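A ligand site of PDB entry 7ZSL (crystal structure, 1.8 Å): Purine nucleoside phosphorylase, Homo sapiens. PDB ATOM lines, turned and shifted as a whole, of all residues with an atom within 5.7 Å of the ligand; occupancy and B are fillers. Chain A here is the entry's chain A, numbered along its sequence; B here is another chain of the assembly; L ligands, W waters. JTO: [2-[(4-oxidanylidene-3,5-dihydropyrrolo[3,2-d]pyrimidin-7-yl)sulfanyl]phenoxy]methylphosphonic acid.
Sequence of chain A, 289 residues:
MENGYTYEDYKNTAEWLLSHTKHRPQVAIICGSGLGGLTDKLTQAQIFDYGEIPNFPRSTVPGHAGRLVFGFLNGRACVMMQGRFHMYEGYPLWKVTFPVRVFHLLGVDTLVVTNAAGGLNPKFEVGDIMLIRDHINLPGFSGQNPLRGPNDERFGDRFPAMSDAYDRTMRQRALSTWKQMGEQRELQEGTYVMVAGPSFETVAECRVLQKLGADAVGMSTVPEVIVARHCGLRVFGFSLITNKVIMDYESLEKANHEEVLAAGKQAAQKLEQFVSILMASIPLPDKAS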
ATOM      1  N   CYS A  31     -34.547  -3.785 -31.962  1.00  0.00           N
ATOM      2  CA  CYS A  31     -33.449  -3.461 -32.913  1.00  0.00           C
ATOM      3  C   CYS A  31     -32.123  -3.571 -32.168  1.00  0.00           C
ATOM      4  O   CYS A  31     -31.914  -2.882 -31.173  1.00  0.00           O
ATOM      5  CB  CYS A  31     -33.637  -2.101 -33.563  1.00  0.00           C
ATOM      6  SG  CYS A  31     -35.144  -1.975 -34.556  1.00  0.00           S
ATOM      7  N   GLY A  32     -31.281  -4.490 -32.650  1.00  0.00           N
ATOM      8  CA  GLY A  32     -29.883  -4.649 -32.217  1.00  0.00           C
ATOM      9  C   GLY A  32     -28.950  -3.881 -33.126  1.00  0.00           C
ATOM     10  O   GLY A  32     -29.416  -3.002 -33.870  1.00  0.00           O
ATOM     11  N   SER A  33     -27.650  -4.190 -33.024  1.00  0.00           N
ATOM     12  CA  SER A  33     -26.547  -3.500 -33.741  1.00  0.00           C
ATOM     13  C   SER A  33     -26.781  -3.590 -35.253  1.00  0.00           C
ATOM     14  O   SER A  33     -27.073  -4.685 -35.736  1.00  0.00           O
ATOM     15  CB  SER A  33     -25.245  -4.091 -33.328  1.00  0.00           C
ATOM     16  OG  SER A  33     -25.116  -4.053 -31.900  1.00  0.00           O
ATOM     17  N   ARG A  84     -32.230  -0.690 -26.588  1.00  0.00           N
ATOM     18  CA  ARG A  84     -32.739  -1.756 -25.694  1.00  0.00           C
ATOM     19  C   ARG A  84     -31.969  -1.673 -24.377  1.00  0.00           C
ATOM     20  O   ARG A  84     -30.889  -1.111 -24.374  1.00  0.00           O
ATOM     21  CB  ARG A  84     -32.674  -3.122 -26.384  1.00  0.00           C
ATOM     22  CG  ARG A  84     -31.313  -3.523 -26.888  1.00  0.00           C
ATOM     23  CD  ARG A  84     -30.882  -4.853 -26.326  1.00  0.00           C
ATOM     24  NE  ARG A  84     -31.657  -5.991 -26.831  1.00  0.00           N
ATOM     25  CZ  ARG A  84     -31.454  -6.588 -27.990  1.00  0.00           C
ATOM     26  NH1 ARG A  84     -32.233  -7.584 -28.322  1.00  0.00           N
ATOM     27  NH2 ARG A  84     -30.597  -6.093 -28.876  1.00  0.00           N
ATOM     28  N   HIS A  86     -30.015  -3.381 -21.090  1.00  0.00           N
ATOM     29  CA  HIS A  86     -29.051  -4.491 -20.949  1.00  0.00           C
ATOM     30  C   HIS A  86     -28.708  -4.711 -19.475  1.00  0.00           C
ATOM     31  O   HIS A  86     -28.638  -3.768 -18.732  1.00  0.00           O
ATOM     32  CB  HIS A  86     -27.745  -4.169 -21.667  1.00  0.00           C
ATOM     33  CG  HIS A  86     -27.843  -3.839 -23.115  1.00  0.00           C
ATOM     34  ND1 HIS A  86     -28.024  -2.566 -23.558  1.00  0.00           N
ATOM     35  CD2 HIS A  86     -27.754  -4.608 -24.212  1.00  0.00           C
ATOM     36  CE1 HIS A  86     -28.068  -2.565 -24.865  1.00  0.00           C
ATOM     37  NE2 HIS A  86     -27.909  -3.808 -25.284  1.00  0.00           N
ATOM     38  N   TYR A  88     -25.881  -5.401 -18.253  1.00  0.00           N
ATOM     39  CA  TYR A  88     -24.576  -4.763 -17.891  1.00  0.00           C
ATOM     40  C   TYR A  88     -24.807  -3.288 -17.484  1.00  0.00           C
ATOM     41  O   TYR A  88     -23.926  -2.753 -16.825  1.00  0.00           O
ATOM     42  CB  TYR A  88     -23.532  -4.840 -18.996  1.00  0.00           C
ATOM     43  CG  TYR A  88     -23.908  -4.247 -20.327  1.00  0.00           C
ATOM     44  CD1 TYR A  88     -23.976  -2.878 -20.538  1.00  0.00           C
ATOM     45  CD2 TYR A  88     -24.129  -5.065 -21.415  1.00  0.00           C
ATOM     46  CE1 TYR A  88     -24.314  -2.342 -21.768  1.00  0.00           C
ATOM     47  CE2 TYR A  88     -24.476  -4.556 -22.652  1.00  0.00           C
ATOM     48  CZ  TYR A  88     -24.568  -3.194 -22.837  1.00  0.00           C
ATOM     49  OH  TYR A  88     -24.896  -2.757 -24.075  1.00  0.00           O
ATOM     50  N   THR A 114     -33.023  -8.696 -32.636  1.00  0.00           N
ATOM     51  CA  THR A 114     -31.700  -8.683 -33.305  1.00  0.00           C
ATOM     52  C   THR A 114     -30.626  -8.261 -32.302  1.00  0.00           C
ATOM     53  O   THR A 114     -30.951  -7.585 -31.298  1.00  0.00           O
ATOM     54  CB  THR A 114     -31.689  -7.856 -34.589  1.00  0.00           C
ATOM     55  OG1 THR A 114     -31.787  -6.498 -34.165  1.00  0.00           O
ATOM     56  CG2 THR A 114     -32.780  -8.236 -35.552  1.00  0.00           C
ATOM     57  N   ASN A 115     -29.405  -8.633 -32.571  1.00  0.00           N
ATOM     58  CA  ASN A 115     -28.253  -8.231 -31.735  1.00  0.00           C
ATOM     59  C   ASN A 115     -26.960  -8.254 -32.525  1.00  0.00           C
ATOM     60  O   ASN A 115     -26.958  -8.686 -33.725  1.00  0.00           O
ATOM     61  CB  ASN A 115     -28.173  -9.105 -30.482  1.00  0.00           C
ATOM     62  CG  ASN A 115     -28.006 -10.578 -30.833  1.00  0.00           C
ATOM     63  OD1 ASN A 115     -27.142 -10.912 -31.601  1.00  0.00           O
ATOM     64  ND2 ASN A 115     -28.791 -11.435 -30.236  1.00  0.00           N
ATOM     65  N   ALA A 116     -25.892  -7.810 -31.859  1.00  0.00           N
ATOM     66  CA  ALA A 116     -24.505  -8.060 -32.286  1.00  0.00           C
ATOM     67  C   ALA A 116     -24.001  -9.270 -31.519  1.00  0.00           C
ATOM     68  O   ALA A 116     -24.429  -9.521 -30.391  1.00  0.00           O
ATOM     69  CB  ALA A 116     -23.639  -6.834 -32.024  1.00  0.00           C
ATOM     70  N   ALA A 117     -23.086 -10.033 -32.110  1.00  0.00           N
ATOM     71  CA  ALA A 117     -22.446 -11.151 -31.395  1.00  0.00           C
ATOM     72  C   ALA A 117     -21.009 -11.310 -31.865  1.00  0.00           C
ATOM     73  O   ALA A 117     -20.683 -10.973 -33.020  1.00  0.00           O
ATOM     74  CB  ALA A 117     -23.233 -12.401 -31.567  1.00  0.00           C
ATOM     75  N   GLY A 118     -20.165 -11.804 -30.972  1.00  0.00           N
ATOM     76  CA  GLY A 118     -18.849 -12.323 -31.305  1.00  0.00           C
ATOM     77  C   GLY A 118     -18.953 -13.709 -31.899  1.00  0.00           C
ATOM     78  O   GLY A 118     -19.634 -14.530 -31.324  1.00  0.00           O
ATOM     79  N   GLY A 119     -18.231 -13.977 -32.983  1.00  0.00           N
ATOM     80  CA  GLY A 119     -18.140 -15.312 -33.622  1.00  0.00           C
ATOM     81  C   GLY A 119     -17.286 -16.293 -32.814  1.00  0.00           C
ATOM     82  O   GLY A 119     -16.093 -16.044 -32.630  1.00  0.00           O
ATOM     83  N   TYR A 192     -26.857 -19.036 -29.855  1.00  0.00           N
ATOM     84  CA  TYR A 192     -26.397 -17.798 -29.197  1.00  0.00           C
ATOM     85  C   TYR A 192     -26.264 -18.083 -27.692  1.00  0.00           C
ATOM     86  O   TYR A 192     -27.225 -18.558 -27.108  1.00  0.00           O
ATOM     87  CB  TYR A 192     -27.423 -16.693 -29.451  1.00  0.00           C
ATOM     88  CG  TYR A 192     -27.189 -15.361 -28.797  1.00  0.00           C
ATOM     89  CD1 TYR A 192     -26.447 -14.371 -29.435  1.00  0.00           C
ATOM     90  CD2 TYR A 192     -27.820 -15.032 -27.614  1.00  0.00           C
ATOM     91  CE1 TYR A 192     -26.299 -13.100 -28.875  1.00  0.00           C
ATOM     92  CE2 TYR A 192     -27.650 -13.777 -27.034  1.00  0.00           C
ATOM     93  CZ  TYR A 192     -26.909 -12.802 -27.673  1.00  0.00           C
ATOM     94  OH  TYR A 192     -26.784 -11.565 -27.105  1.00  0.00           O
ATOM     95  N   VAL A 195     -23.937 -13.900 -22.198  1.00  0.00           N
ATOM     96  CA  VAL A 195     -23.108 -13.583 -20.994  1.00  0.00           C
ATOM     97  C   VAL A 195     -23.515 -12.161 -20.562  1.00  0.00           C
ATOM     98  O   VAL A 195     -24.008 -11.388 -21.423  1.00  0.00           O
ATOM     99  CB  VAL A 195     -21.614 -13.725 -21.300  1.00  0.00           C
ATOM    100  CG1 VAL A 195     -21.261 -15.159 -21.704  1.00  0.00           C
ATOM    101  CG2 VAL A 195     -21.163 -12.754 -22.367  1.00  0.00           C
ATOM    102  N   PHE A 200     -15.320  -7.947 -22.448  1.00  0.00           N
ATOM    103  CA  PHE A 200     -15.187  -9.028 -23.452  1.00  0.00           C
ATOM    104  C   PHE A 200     -14.477 -10.246 -22.842  1.00  0.00           C
ATOM    105  O   PHE A 200     -13.762 -10.097 -21.832  1.00  0.00           O
ATOM    106  CB  PHE A 200     -14.454  -8.510 -24.694  1.00  0.00           C
ATOM    107  CG  PHE A 200     -15.230  -7.547 -25.546  1.00  0.00           C
ATOM    108  CD1 PHE A 200     -16.201  -8.016 -26.428  1.00  0.00           C
ATOM    109  CD2 PHE A 200     -14.977  -6.190 -25.500  1.00  0.00           C
ATOM    110  CE1 PHE A 200     -16.909  -7.123 -27.246  1.00  0.00           C
ATOM    111  CE2 PHE A 200     -15.703  -5.297 -26.297  1.00  0.00           C
ATOM    112  CZ  PHE A 200     -16.620  -5.777 -27.196  1.00  0.00           C
ATOM    113  N   GLU A 201     -14.560 -11.375 -23.518  1.00  0.00           N
ATOM    114  CA  GLU A 201     -14.137 -12.697 -22.992  1.00  0.00           C
ATOM    115  C   GLU A 201     -12.622 -12.842 -23.080  1.00  0.00           C
ATOM    116  O   GLU A 201     -12.006 -12.306 -24.039  1.00  0.00           O
ATOM    117  CB  GLU A 201     -14.817 -13.830 -23.753  1.00  0.00           C
ATOM    118  CG  GLU A 201     -16.299 -13.870 -23.527  1.00  0.00           C
ATOM    119  CD  GLU A 201     -17.077 -12.853 -24.325  1.00  0.00           C
ATOM    120  OE1 GLU A 201     -16.667 -12.543 -25.472  1.00  0.00           O
ATOM    121  OE2 GLU A 201     -18.058 -12.317 -23.779  1.00  0.00           O
ATOM    122  N   VAL A 217     -21.557 -15.284 -29.242  1.00  0.00           N
ATOM    123  CA  VAL A 217     -21.736 -14.783 -27.850  1.00  0.00           C
ATOM    124  C   VAL A 217     -22.196 -13.315 -27.911  1.00  0.00           C
ATOM    125  O   VAL A 217     -21.587 -12.510 -28.663  1.00  0.00           O
ATOM    126  CB  VAL A 217     -20.467 -14.950 -27.002  1.00  0.00           C
ATOM    127  CG1 VAL A 217     -19.238 -14.288 -27.608  1.00  0.00           C
ATOM    128  CG2 VAL A 217     -20.678 -14.442 -25.573  1.00  0.00           C
ATOM    129  N   GLY A 218     -23.083 -12.958 -26.994  1.00  0.00           N
ATOM    130  CA  GLY A 218     -23.499 -11.551 -26.854  1.00  0.00           C
ATOM    131  C   GLY A 218     -24.093 -11.296 -25.494  1.00  0.00           C
ATOM    132  O   GLY A 218     -24.017 -12.189 -24.632  1.00  0.00           O
ATOM    133  N   MET A 219     -24.707 -10.125 -25.326  1.00  0.00           N
ATOM    134  CA  MET A 219     -25.018  -9.621 -23.967  1.00  0.00           C
ATOM    135  C   MET A 219     -26.489  -9.232 -23.853  1.00  0.00           C
ATOM    136  O   MET A 219     -26.806  -8.445 -22.950  1.00  0.00           O
ATOM    137  CB  MET A 219     -24.135  -8.412 -23.651  1.00  0.00           C
ATOM    138  CG  MET A 219     -22.682  -8.724 -23.555  1.00  0.00           C
ATOM    139  SD  MET A 219     -21.606  -7.217 -23.404  1.00  0.00           S
ATOM    140  CE  MET A 219     -20.042  -7.923 -23.902  1.00  0.00           C
ATOM    141  N   SER A 220     -27.361  -9.810 -24.664  1.00  0.00           N
ATOM    142  CA  SER A 220     -28.805  -9.441 -24.612  1.00  0.00           C
ATOM    143  C   SER A 220     -29.686 -10.611 -25.031  1.00  0.00           C
ATOM    144  O   SER A 220     -29.176 -11.766 -25.064  1.00  0.00           O
ATOM    145  CB  SER A 220     -29.040  -8.240 -25.470  1.00  0.00           C
ATOM    146  OG  SER A 220     -28.909  -8.596 -26.851  1.00  0.00           O
ATOM    147  N   THR A 221     -30.951 -10.281 -25.367  1.00  0.00           N
ATOM    148  CA  THR A 221     -31.822 -11.097 -26.267  1.00  0.00           C
ATOM    149  C   THR A 221     -32.456 -12.235 -25.482  1.00  0.00           C
ATOM    150  O   THR A 221     -33.666 -12.367 -25.542  1.00  0.00           O
ATOM    151  CB  THR A 221     -31.046 -11.582 -27.497  1.00  0.00           C
ATOM    152  OG1 THR A 221     -30.618 -10.420 -28.200  1.00  0.00           O
ATOM    153  CG2 THR A 221     -31.861 -12.480 -28.411  1.00  0.00           C
ATOM    154  N   THR A 242     -20.020  -9.348 -35.483  1.00  0.00           N
ATOM    155  CA  THR A 242     -19.294  -8.069 -35.554  1.00  0.00           C
ATOM    156  C   THR A 242     -17.791  -8.321 -35.462  1.00  0.00           C
ATOM    157  O   THR A 242     -17.019  -7.394 -35.854  1.00  0.00           O
ATOM    158  CB  THR A 242     -19.824  -7.119 -34.484  1.00  0.00           C
ATOM    159  OG1 THR A 242     -19.671  -7.786 -33.227  1.00  0.00           O
ATOM    160  CG2 THR A 242     -21.249  -6.725 -34.737  1.00  0.00           C
ATOM    161  N   ASN A 243     -17.365  -9.478 -34.964  1.00  0.00           N
ATOM    162  CA  ASN A 243     -15.941  -9.768 -34.667  1.00  0.00           C
ATOM    163  C   ASN A 243     -15.780 -11.259 -34.409  1.00  0.00           C
ATOM    164  O   ASN A 243     -16.759 -11.918 -33.978  1.00  0.00           O
ATOM    165  CB  ASN A 243     -15.429  -8.939 -33.482  1.00  0.00           C
ATOM    166  CG  ASN A 243     -16.171  -9.252 -32.205  1.00  0.00           C
ATOM    167  OD1 ASN A 243     -17.368  -9.016 -32.100  1.00  0.00           O
ATOM    168  ND2 ASN A 243     -15.445  -9.770 -31.227  1.00  0.00           N
ATOM    169  N   VAL A 245     -14.081 -13.806 -31.994  1.00  0.00           N
ATOM    170  CA  VAL A 245     -13.543 -13.740 -30.599  1.00  0.00           C
ATOM    171  C   VAL A 245     -12.136 -14.312 -30.633  1.00  0.00           C
ATOM    172  O   VAL A 245     -11.887 -15.211 -31.443  1.00  0.00           O
ATOM    173  CB  VAL A 245     -14.482 -14.426 -29.584  1.00  0.00           C
ATOM    174  CG1 VAL A 245     -15.879 -13.781 -29.581  1.00  0.00           C
ATOM    175  CG2 VAL A 245     -14.568 -15.900 -29.800  1.00  0.00           C
ATOM    176  N   ALA A 255     -10.838  -7.503 -28.871  1.00  0.00           N
ATOM    177  CA  ALA A 255     -12.237  -7.105 -29.092  1.00  0.00           C
ATOM    178  C   ALA A 255     -12.397  -5.697 -28.562  1.00  0.00           C
ATOM    179  O   ALA A 255     -11.821  -5.378 -27.480  1.00  0.00           O
ATOM    180  CB  ALA A 255     -13.153  -8.091 -28.410  1.00  0.00           C
ATOM    181  N   HIS A 257     -15.381  -2.098 -28.669  1.00  0.00           N
ATOM    182  CA  HIS A 257     -16.722  -1.565 -29.001  1.00  0.00           C
ATOM    183  C   HIS A 257     -16.681  -0.844 -30.362  1.00  0.00           C
ATOM    184  O   HIS A 257     -17.668  -0.900 -31.086  1.00  0.00           O
ATOM    185  CB  HIS A 257     -17.258  -0.622 -27.908  1.00  0.00           C
ATOM    186  CG  HIS A 257     -18.707  -0.342 -28.104  1.00  0.00           C
ATOM    187  ND1 HIS A 257     -19.278   0.893 -27.842  1.00  0.00           N
ATOM    188  CD2 HIS A 257     -19.704  -1.124 -28.587  1.00  0.00           C
ATOM    189  CE1 HIS A 257     -20.564   0.855 -28.152  1.00  0.00           C
ATOM    190  NE2 HIS A 257     -20.860  -0.390 -28.588  1.00  0.00           N
ATOM    191  N   VAL A 260     -17.275  -3.198 -33.131  1.00  0.00           N
ATOM    192  CA  VAL A 260     -18.704  -3.632 -33.058  1.00  0.00           C
ATOM    193  C   VAL A 260     -19.556  -2.571 -33.753  1.00  0.00           C
ATOM    194  O   VAL A 260     -20.379  -2.946 -34.609  1.00  0.00           O
ATOM    195  CB  VAL A 260     -19.156  -3.874 -31.600  1.00  0.00           C
ATOM    196  CG1 VAL A 260     -20.639  -4.172 -31.494  1.00  0.00           C
ATOM    197  CG2 VAL A 260     -18.354  -4.979 -30.959  1.00  0.00           C
ATOM    198  N   PHE B 159     -16.752  -1.198 -22.469  1.00  0.00           N
ATOM    199  CA  PHE B 159     -16.603  -2.639 -22.855  1.00  0.00           C
ATOM    200  C   PHE B 159     -15.124  -2.949 -23.029  1.00  0.00           C
ATOM    201  O   PHE B 159     -14.662  -3.161 -24.147  1.00  0.00           O
ATOM    202  CB  PHE B 159     -17.406  -2.963 -24.120  1.00  0.00           C
ATOM    203  CG  PHE B 159     -18.855  -2.542 -24.102  1.00  0.00           C
ATOM    204  CD1 PHE B 159     -19.821  -3.304 -23.441  1.00  0.00           C
ATOM    205  CD2 PHE B 159     -19.257  -1.367 -24.730  1.00  0.00           C
ATOM    206  CE1 PHE B 159     -21.147  -2.900 -23.398  1.00  0.00           C
ATOM    207  CE2 PHE B 159     -20.583  -0.955 -24.716  1.00  0.00           C
ATOM    208  CZ  PHE B 159     -21.531  -1.725 -24.047  1.00  0.00           C
HETATM  209  C2  JTO L   1     -17.934 -10.487 -28.220  1.00  0.00           C
HETATM  210  C4  JTO L   1     -19.357 -10.675 -26.255  1.00  0.00           C
HETATM  211  C6  JTO L   1     -20.157  -9.406 -27.948  1.00  0.00           C
HETATM  212  C12 JTO L   1     -21.502  -3.658 -26.906  1.00  0.00           C
HETATM  213  C13 JTO L   1     -22.799  -4.037 -27.200  1.00  0.00           C
HETATM  214  C14 JTO L   1     -23.116  -5.337 -27.634  1.00  0.00           C
HETATM  215  C16 JTO L   1     -25.481  -4.843 -27.666  1.00  0.00           C
HETATM  216  C21 JTO L   1     -20.263  -8.334 -29.976  1.00  0.00           C
HETATM  217  C23 JTO L   1     -18.981  -9.675 -28.742  1.00  0.00           C
HETATM  218  O20 JTO L   1     -27.004  -7.058 -27.460  1.00  0.00           O
HETATM  219  P17 JTO L   1     -26.868  -5.694 -28.247  1.00  0.00           P
HETATM  220  O18 JTO L   1     -27.961  -4.653 -28.057  1.00  0.00           O
HETATM  221  O19 JTO L   1     -26.863  -5.930 -29.714  1.00  0.00           O
HETATM  222  O15 JTO L   1     -24.394  -5.753 -27.939  1.00  0.00           O
HETATM  223  C11 JTO L   1     -20.468  -4.595 -27.093  1.00  0.00           C
HETATM  224  C10 JTO L   1     -20.804  -5.887 -27.536  1.00  0.00           C
HETATM  225  C9  JTO L   1     -22.117  -6.314 -27.833  1.00  0.00           C
HETATM  226  S8  JTO L   1     -22.491  -7.881 -28.417  1.00  0.00           S
HETATM  227  C7  JTO L   1     -20.998  -8.582 -28.760  1.00  0.00           C
HETATM  228  N22 JTO L   1     -19.095  -8.999 -29.964  1.00  0.00           N
HETATM  229  O1  JTO L   1     -16.840 -10.751 -28.832  1.00  0.00           O
HETATM  230  N5  JTO L   1     -20.350  -9.926 -26.708  1.00  0.00           N
HETATM  231  N3  JTO L   1     -18.201 -10.997 -26.942  1.00  0.00           N
HETATM  232  O   HOH W   1     -14.667 -11.407 -27.142  1.00  0.00           O
HETATM  233  O   HOH W   2     -25.770  -9.265 -28.162  1.00  0.00           O
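Water W2 lies within hydrogen-bond range of the backbone carbonyl oxygen (O) of Ala 116, an oxygen (O20) of the ligand, the side-chain hydroxyl (OH) of Tyr 192, the backbone NH (N) of Met 219 and the side-chain hydroxyl (OG) of Ser 220.
Water W1 bridges an oxygen (O1) of the ligand and the side-chain carboxylate (OE1) of Glu 201.
The guanidinium group (NH2) of Arg 84 sits at hydrogen-bond distance from the backbone carbonyl oxygen (O) of Thr 114, 2.9 Å away.
The backbone carbonyl oxygen (O) of Arg 84 sits close to a ring nitrogen (ND1) of His 86.
NH1 of Arg 84 lies within hydrogen-bond range of OG1 of Thr 221.
O of Gly 119 lies within hydrogen-bond range of N of Val 245, 3.1 Å away.
A ring nitrogen (ND1) of His 86 is in hydrogen-bond range of the side-chain hydroxyl (OH) of Tyr 88, at 3.2 Å.
OG of Ser 220 is in hydrogen-bond range of OG1 of Thr 221 (2.8 Å).
ND2 of Asn 115 sits at hydrogen-bond distance from OG1 of Thr 221 (2.9 Å).
The side-chain hydroxyl (OH) of Tyr 192 lies within hydrogen-bond range of the backbone NH (N) of Met 219 (3.1 Å).
Tyr 88 touches the ligand (OH to C13, 3.98 Å).
Asn 115 touches the ligand.
Ala 117 touches the ligand.
Phe 200 touches the ligand.
CA of Gly 218 touches N5 of the ligand, at 3.5 Å.
Met 219 touches the ligand (CE to N5, 3.5 Å).
Thr 242 touches the ligand (OG1 to C21, 3.3 Å).
Val 245 touches the ligand (CG1 to O1, 3.3 Å).
His 257 touches the ligand (CD2 to C12, 3.5 Å).
CG2 of Val 260 touches C21 of the ligand (3.98 Å).
Phe 159 of chain B touches the ligand (CZ to C12, 3.5 Å).
Hydrophobic or aromatic side chains within 4 Å of the ligand: His 86, Ala 116, Phe 200, Val 217, Met 219, Val 245, His 257, Val 260 and Phe 159 of chain B.
Within 4 Å of the ligand: Ser 33, Arg 84, His 86, Tyr 88, Asn 115, Ala 116, Ala 117, Gly 118, Phe 200, Glu 201, Val 217, Gly 218, Met 219, Ser 220, Thr 242, Asn 243, Val 245, His 257, Val 260 and Phe 159 of chain B.
The side-chain amide oxygen (OD1) of Asn 243 lies within hydrogen-bond range of a nitrogen (N22) of the ligand, at 2.7 Å.
The backbone carbonyl oxygen (O) of Val 217 sits close to a nitrogen (N5) of the ligand (3.5 Å).
O18 of the ligand is in salt-bridge range of NH2 of Arg 84 (3.1 Å).
N of Ala 116 is in hydrogen-bond range of O19 of the ligand, at 3.0 Å.
OG of Ser 220 is in hydrogen-bond range of O20 of the ligand (2.5 Å).
An oxygen (O19) of the ligand is in hydrogen-bond range of the side-chain hydroxyl of Ser 33, at 3.4 Å.
The side-chain carboxylate (OE1) of Glu 201 sits at hydrogen-bond distance from a nitrogen (N3) of the ligand.
A ring nitrogen (NE2) of His 86 is in hydrogen-bond range of an oxygen (O18) of the ligand (2.9 Å).
The backbone NH of Gly 118 lies close to a nitrogen (N22) of the ligand (3.2 Å).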
